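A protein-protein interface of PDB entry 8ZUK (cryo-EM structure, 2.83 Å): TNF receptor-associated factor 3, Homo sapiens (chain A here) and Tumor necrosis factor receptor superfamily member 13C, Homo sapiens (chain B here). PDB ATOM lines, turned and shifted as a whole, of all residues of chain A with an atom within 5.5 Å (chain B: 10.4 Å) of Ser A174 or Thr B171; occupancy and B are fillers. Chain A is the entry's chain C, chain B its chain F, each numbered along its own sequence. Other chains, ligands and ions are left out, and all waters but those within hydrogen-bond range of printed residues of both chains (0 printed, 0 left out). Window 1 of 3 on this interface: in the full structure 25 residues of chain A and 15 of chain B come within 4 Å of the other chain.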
ATOM      1  N   THR A 172      13.105  12.829 -22.313  1.00  0.00           N
ATOM      2  CA  THR A 172      11.850  12.220 -22.756  1.00  0.00           C
ATOM      3  C   THR A 172      12.148  11.421 -24.020  1.00  0.00           C
ATOM      4  O   THR A 172      12.323  11.996 -25.099  1.00  0.00           O
ATOM      5  CB  THR A 172      10.776  13.273 -23.006  1.00  0.00           C
ATOM      6  OG1 THR A 172      10.523  13.996 -21.794  1.00  0.00           O
ATOM      7  CG2 THR A 172       9.487  12.618 -23.474  1.00  0.00           C
ATOM      8  N   LEU A 173      12.207  10.096 -23.882  1.00  0.00           N
ATOM      9  CA  LEU A 173      12.574   9.252 -25.015  1.00  0.00           C
ATOM     10  C   LEU A 173      11.454   9.176 -26.045  1.00  0.00           C
ATOM     11  O   LEU A 173      11.711   9.252 -27.253  1.00  0.00           O
ATOM     12  CB  LEU A 173      12.951   7.853 -24.527  1.00  0.00           C
ATOM     13  CG  LEU A 173      14.262   7.741 -23.748  1.00  0.00           C
ATOM     14  CD1 LEU A 173      14.595   6.285 -23.463  1.00  0.00           C
ATOM     15  CD2 LEU A 173      15.397   8.415 -24.505  1.00  0.00           C
ATOM     16  N   SER A 174      10.210   9.027 -25.596  1.00  0.00           N
ATOM     17  CA  SER A 174       9.089   8.837 -26.502  1.00  0.00           C
ATOM     18  C   SER A 174       7.922   9.716 -26.074  1.00  0.00           C
ATOM     19  O   SER A 174       7.829  10.147 -24.923  1.00  0.00           O
ATOM     20  CB  SER A 174       8.647   7.368 -26.555  1.00  0.00           C
ATOM     21  OG  SER A 174       7.973   6.994 -25.367  1.00  0.00           O
ATOM     22  N   LEU A 175       7.029   9.975 -27.027  1.00  0.00           N
ATOM     23  CA  LEU A 175       5.841  10.785 -26.809  1.00  0.00           C
ATOM     24  C   LEU A 175       4.603   9.979 -27.170  1.00  0.00           C
ATOM     25  O   LEU A 175       4.618   9.194 -28.124  1.00  0.00           O
ATOM     26  CB  LEU A 175       5.887  12.071 -27.641  1.00  0.00           C
ATOM     27  CG  LEU A 175       7.073  13.005 -27.401  1.00  0.00           C
ATOM     28  CD1 LEU A 175       7.130  14.079 -28.473  1.00  0.00           C
ATOM     29  CD2 LEU A 175       6.987  13.630 -26.019  1.00  0.00           C
ATOM     30  N   TYR A 176       3.533  10.178 -26.407  1.00  0.00           N
ATOM     31  CA  TYR A 176       2.274   9.477 -26.616  1.00  0.00           C
ATOM     32  C   TYR A 176       1.223  10.436 -27.159  1.00  0.00           C
ATOM     33  O   TYR A 176       1.073  11.557 -26.664  1.00  0.00           O
ATOM     34  CB  TYR A 176       1.776   8.839 -25.316  1.00  0.00           C
ATOM     35  CG  TYR A 176       2.350   7.467 -25.054  1.00  0.00           C
ATOM     36  CD1 TYR A 176       3.553   7.311 -24.379  1.00  0.00           C
ATOM     37  CD2 TYR A 176       1.690   6.324 -25.487  1.00  0.00           C
ATOM     38  CE1 TYR A 176       4.080   6.057 -24.137  1.00  0.00           C
ATOM     39  CE2 TYR A 176       2.209   5.066 -25.252  1.00  0.00           C
ATOM     40  CZ  TYR A 176       3.404   4.939 -24.577  1.00  0.00           C
ATOM     41  OH  TYR A 176       3.927   3.687 -24.341  1.00  0.00           O
ATOM     42  N   ARG A 192       2.683   6.240 -30.711  1.00  0.00           N
ATOM     43  CA  ARG A 192       3.904   6.511 -29.963  1.00  0.00           C
ATOM     44  C   ARG A 192       5.036   6.805 -30.937  1.00  0.00           C
ATOM     45  O   ARG A 192       5.209   6.083 -31.925  1.00  0.00           O
ATOM     46  CB  ARG A 192       4.270   5.329 -29.063  1.00  0.00           C
ATOM     47  CG  ARG A 192       5.215   5.683 -27.933  1.00  0.00           C
ATOM     48  CD  ARG A 192       5.657   4.437 -27.194  1.00  0.00           C
ATOM     49  NE  ARG A 192       6.584   4.739 -26.111  1.00  0.00           N
ATOM     50  CZ  ARG A 192       7.242   3.824 -25.415  1.00  0.00           C
ATOM     51  NH1 ARG A 192       7.096   2.532 -25.658  1.00  0.00           N
ATOM     52  NH2 ARG A 192       8.074   4.214 -24.454  1.00  0.00           N
ATOM     53  N   VAL A 193       5.807   7.855 -30.657  1.00  0.00           N
ATOM     54  CA  VAL A 193       6.874   8.302 -31.542  1.00  0.00           C
ATOM     55  C   VAL A 193       8.154   8.486 -30.736  1.00  0.00           C
ATOM     56  O   VAL A 193       8.118   8.917 -29.578  1.00  0.00           O
ATOM     57  CB  VAL A 193       6.492   9.610 -32.274  1.00  0.00           C
ATOM     58  CG1 VAL A 193       6.384  10.773 -31.297  1.00  0.00           C
ATOM     59  CG2 VAL A 193       7.490   9.919 -33.376  1.00  0.00           C
ATOM     60  N   TYR A 194       9.284   8.128 -31.343  1.00  0.00           N
ATOM     61  CA  TYR A 194      10.609   8.403 -30.800  1.00  0.00           C
ATOM     62  C   TYR A 194      11.295   9.425 -31.693  1.00  0.00           C
ATOM     63  O   TYR A 194      11.620   9.124 -32.848  1.00  0.00           O
ATOM     64  CB  TYR A 194      11.449   7.131 -30.708  1.00  0.00           C
ATOM     65  CG  TYR A 194      11.064   6.198 -29.585  1.00  0.00           C
ATOM     66  CD1 TYR A 194       9.935   5.399 -29.673  1.00  0.00           C
ATOM     67  CD2 TYR A 194      11.844   6.106 -28.439  1.00  0.00           C
ATOM     68  CE1 TYR A 194       9.588   4.539 -28.650  1.00  0.00           C
ATOM     69  CE2 TYR A 194      11.505   5.251 -27.411  1.00  0.00           C
ATOM     70  CZ  TYR A 194      10.376   4.470 -27.522  1.00  0.00           C
ATOM     71  OH  TYR A 194      10.038   3.617 -26.497  1.00  0.00           O
ATOM     72  N   ALA B 165       8.570  -2.680 -29.589  1.00  0.00           N
ATOM     73  CA  ALA B 165       9.231  -1.506 -29.049  1.00  0.00           C
ATOM     74  C   ALA B 165      10.301  -1.917 -28.041  1.00  0.00           C
ATOM     75  O   ALA B 165      10.518  -3.099 -27.763  1.00  0.00           O
ATOM     76  CB  ALA B 165       8.211  -0.562 -28.412  1.00  0.00           C
ATOM     77  N   THR B 166      10.975  -0.916 -27.486  1.00  0.00           N
ATOM     78  CA  THR B 166      12.041  -1.089 -26.505  1.00  0.00           C
ATOM     79  C   THR B 166      11.749  -0.242 -25.273  1.00  0.00           C
ATOM     80  O   THR B 166      12.568   0.563 -24.826  1.00  0.00           O
ATOM     81  CB  THR B 166      13.401  -0.742 -27.108  1.00  0.00           C
ATOM     82  OG1 THR B 166      13.478  -1.270 -28.438  1.00  0.00           O
ATOM     83  CG2 THR B 166      14.525  -1.354 -26.281  1.00  0.00           C
ATOM     84  N   GLU B 167      10.535  -0.397 -24.739  1.00  0.00           N
ATOM     85  CA  GLU B 167      10.038   0.388 -23.612  1.00  0.00           C
ATOM     86  C   GLU B 167      11.052   0.499 -22.480  1.00  0.00           C
ATOM     87  O   GLU B 167      11.393  -0.499 -21.840  1.00  0.00           O
ATOM     88  CB  GLU B 167       8.743  -0.231 -23.078  1.00  0.00           C
ATOM     89  CG  GLU B 167       8.069   0.574 -21.981  1.00  0.00           C
ATOM     90  CD  GLU B 167       7.235   1.715 -22.524  1.00  0.00           C
ATOM     91  OE1 GLU B 167       6.679   1.565 -23.632  1.00  0.00           O
ATOM     92  OE2 GLU B 167       7.137   2.759 -21.846  1.00  0.00           O
ATOM     93  N   LEU B 168      11.536   1.716 -22.230  1.00  0.00           N
ATOM     94  CA  LEU B 168      12.460   1.988 -21.137  1.00  0.00           C
ATOM     95  C   LEU B 168      11.865   2.947 -20.116  1.00  0.00           C
ATOM     96  O   LEU B 168      11.858   2.654 -18.917  1.00  0.00           O
ATOM     97  CB  LEU B 168      13.781   2.548 -21.688  1.00  0.00           C
ATOM     98  CG  LEU B 168      14.645   1.593 -22.515  1.00  0.00           C
ATOM     99  CD1 LEU B 168      15.856   2.320 -23.076  1.00  0.00           C
ATOM    100  CD2 LEU B 168      15.072   0.397 -21.681  1.00  0.00           C
ATOM    101  N   GLY B 169      11.361   4.092 -20.562  1.00  0.00           N
ATOM    102  CA  GLY B 169      10.776   5.061 -19.654  1.00  0.00           C
ATOM    103  C   GLY B 169      10.767   6.440 -20.289  1.00  0.00           C
ATOM    104  O   GLY B 169      10.941   6.582 -21.498  1.00  0.00           O
ATOM    105  N   SER B 170      10.565   7.443 -19.436  1.00  0.00           N
ATOM    106  CA  SER B 170      10.525   8.848 -19.842  1.00  0.00           C
ATOM    107  C   SER B 170       9.487   9.067 -20.944  1.00  0.00           C
ATOM    108  O   SER B 170       9.796   9.485 -22.061  1.00  0.00           O
ATOM    109  CB  SER B 170      11.911   9.328 -20.282  1.00  0.00           C
ATOM    110  OG  SER B 170      12.825   9.305 -19.200  1.00  0.00           O
ATOM    111  N   THR B 171       8.235   8.773 -20.604  1.00  0.00           N
ATOM    112  CA  THR B 171       7.116   8.894 -21.527  1.00  0.00           C
ATOM    113  C   THR B 171       6.208  10.025 -21.071  1.00  0.00           C
ATOM    114  O   THR B 171       5.735  10.023 -19.930  1.00  0.00           O
ATOM    115  CB  THR B 171       6.324   7.586 -21.610  1.00  0.00           C
ATOM    116  OG1 THR B 171       6.001   7.138 -20.288  1.00  0.00           O
ATOM    117  CG2 THR B 171       7.143   6.514 -22.310  1.00  0.00           C
ATOM    118  N   GLU B 172       5.968  10.985 -21.962  1.00  0.00           N
ATOM    119  CA  GLU B 172       5.098  12.120 -21.673  1.00  0.00           C
ATOM    120  C   GLU B 172       4.121  12.286 -22.824  1.00  0.00           C
ATOM    121  O   GLU B 172       4.537  12.530 -23.960  1.00  0.00           O
ATOM    122  CB  GLU B 172       5.904  13.407 -21.467  1.00  0.00           C
ATOM    123  CG  GLU B 172       7.194  13.232 -20.681  1.00  0.00           C
ATOM    124  CD  GLU B 172       6.953  13.062 -19.195  1.00  0.00           C
ATOM    125  OE1 GLU B 172       5.873  13.468 -18.716  1.00  0.00           O
ATOM    126  OE2 GLU B 172       7.844  12.523 -18.505  1.00  0.00           O
ATOM    127  N   LEU B 173       2.830  12.149 -22.530  1.00  0.00           N
ATOM    128  CA  LEU B 173       1.810  12.373 -23.547  1.00  0.00           C
ATOM    129  C   LEU B 173       1.776  13.846 -23.932  1.00  0.00           C
ATOM    130  O   LEU B 173       1.728  14.724 -23.066  1.00  0.00           O
ATOM    131  CB  LEU B 173       0.443  11.923 -23.029  1.00  0.00           C
ATOM    132  CG  LEU B 173      -0.721  11.891 -24.023  1.00  0.00           C
ATOM    133  CD1 LEU B 173      -1.617  10.696 -23.748  1.00  0.00           C
ATOM    134  CD2 LEU B 173      -1.530  13.181 -23.964  1.00  0.00           C
ATOM    135  N   VAL B 174       1.804  14.114 -25.234  1.00  0.00           N
ATOM    136  CA  VAL B 174       1.790  15.477 -25.751  1.00  0.00           C
ATOM    137  C   VAL B 174       0.664  15.606 -26.771  1.00  0.00           C
ATOM    138  O   VAL B 174       0.552  14.788 -27.692  1.00  0.00           O
ATOM    139  CB  VAL B 174       3.148  15.887 -26.353  1.00  0.00           C
ATOM    140  CG1 VAL B 174       3.498  15.055 -27.582  1.00  0.00           C
ATOM    141  CG2 VAL B 174       3.139  17.366 -26.695  1.00  0.00           C
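The guanidinium group (NE) of Arg A192 lies within hydrogen-bond range of the side-chain hydroxyl (OG) of Ser A174 (2.8 Å). N of Leu A175 sits at hydrogen-bond distance from O of Val A193 (3.0 Å). The side-chain hydroxyl of Tyr A176 sits at hydrogen-bond distance from the guanidinium group of Arg A192 (3.4 Å). OH of Tyr A194 is in hydrogen-bond range of NH2 of Arg A192, at 2.9 Å.
Glu B172 touches Thr A172. Gly B169 touches Leu A173. O of Ser B170 touches O of Ser A174, 3.5 Å away. Ser A174 touches Thr B171 (OG to CG2, 3.2 Å). N of Glu B172 touches O of Ser A174, 3.6 Å away. O of Glu B172 touches CD2 of Leu A175 (3.4 Å). CG1 of Val B174 touches CB of Leu A175, at 3.8 Å. Glu B167 touches Tyr A176. N of Tyr A176 touches O of Glu B172 (3.5 Å). Tyr A176 touches Leu B173 (O to CG, 3.2 Å).
Of the 10 printed residues of chain B, 7 touch a printed residue of chain A. Of the 8 printed residues of chain A, 6 touch a printed residue of chain B. Hydrophobic or aromatic side chains of chain A that line the printed part of chain B: Leu A173, Leu A175 and Tyr A176. Along chain A the printed residues that touch a printed residue of chain B span positions 172 to 192. Among the printed residues, 16 pairs touch across the chains. Among the printed residues, Asp or Glu carboxylates within 4 Å of a Lys or Arg side-chain nitrogen of the other chain: Arg A192 with Glu B167 (2.3 Å).
The backbone NH of Leu A173 sits at hydrogen-bond distance from the backbone carbonyl oxygen of Ser B170. The backbone carbonyl oxygen (O) of Tyr A176 is in hydrogen-bond range of the backbone NH (N) of Val B174, at 3.0 Å. The guanidinium group (NH2) of Arg A192 lies within salt-bridge range of the side-chain carboxylate (OE1) of Glu B167 (3.1 Å).
Leu A173 touches just these residues of chain B: Gly B169 and Ser B170. Of chain B, only Ser B170 (3.5 Å), Thr B171 (3.2 Å) and Glu B172 (3.6 Å) come within 4 Å of Ser A174. Of chain B, only Glu B172 (3.4 Å) and Val B174 (3.8 Å) come within 4 Å of Leu A175. Of the printed residues of chain B, Tyr A176 touches Glu B167, Thr B171, Glu B172, Leu B173 and Val B174. Ala B165 touches none of the printed residues of chain A. Printed residues of chain A within 4 Å of Gly B169: Leu A173 (3.9 Å). Printed residues of chain A within 4 Å of Ser B170: Thr A172, Leu A173 and Ser A174. Of chain A, only Ser A174, Tyr A176 and Arg A192 come within 4 Å of Thr B171. Printed residues of chain A within 4 Å of Glu B172: Thr A172, Ser A174, Leu A175 and Tyr A176. Printed residues of chain A within 4 Å of Leu B173: Tyr A176. The nearest residue of chain A that does not touch Thr B171 is Thr A172 (4.8 Å). The nearest printed residue of chain B that does not touch Tyr A176 is Ser B170 (7.0 Å).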
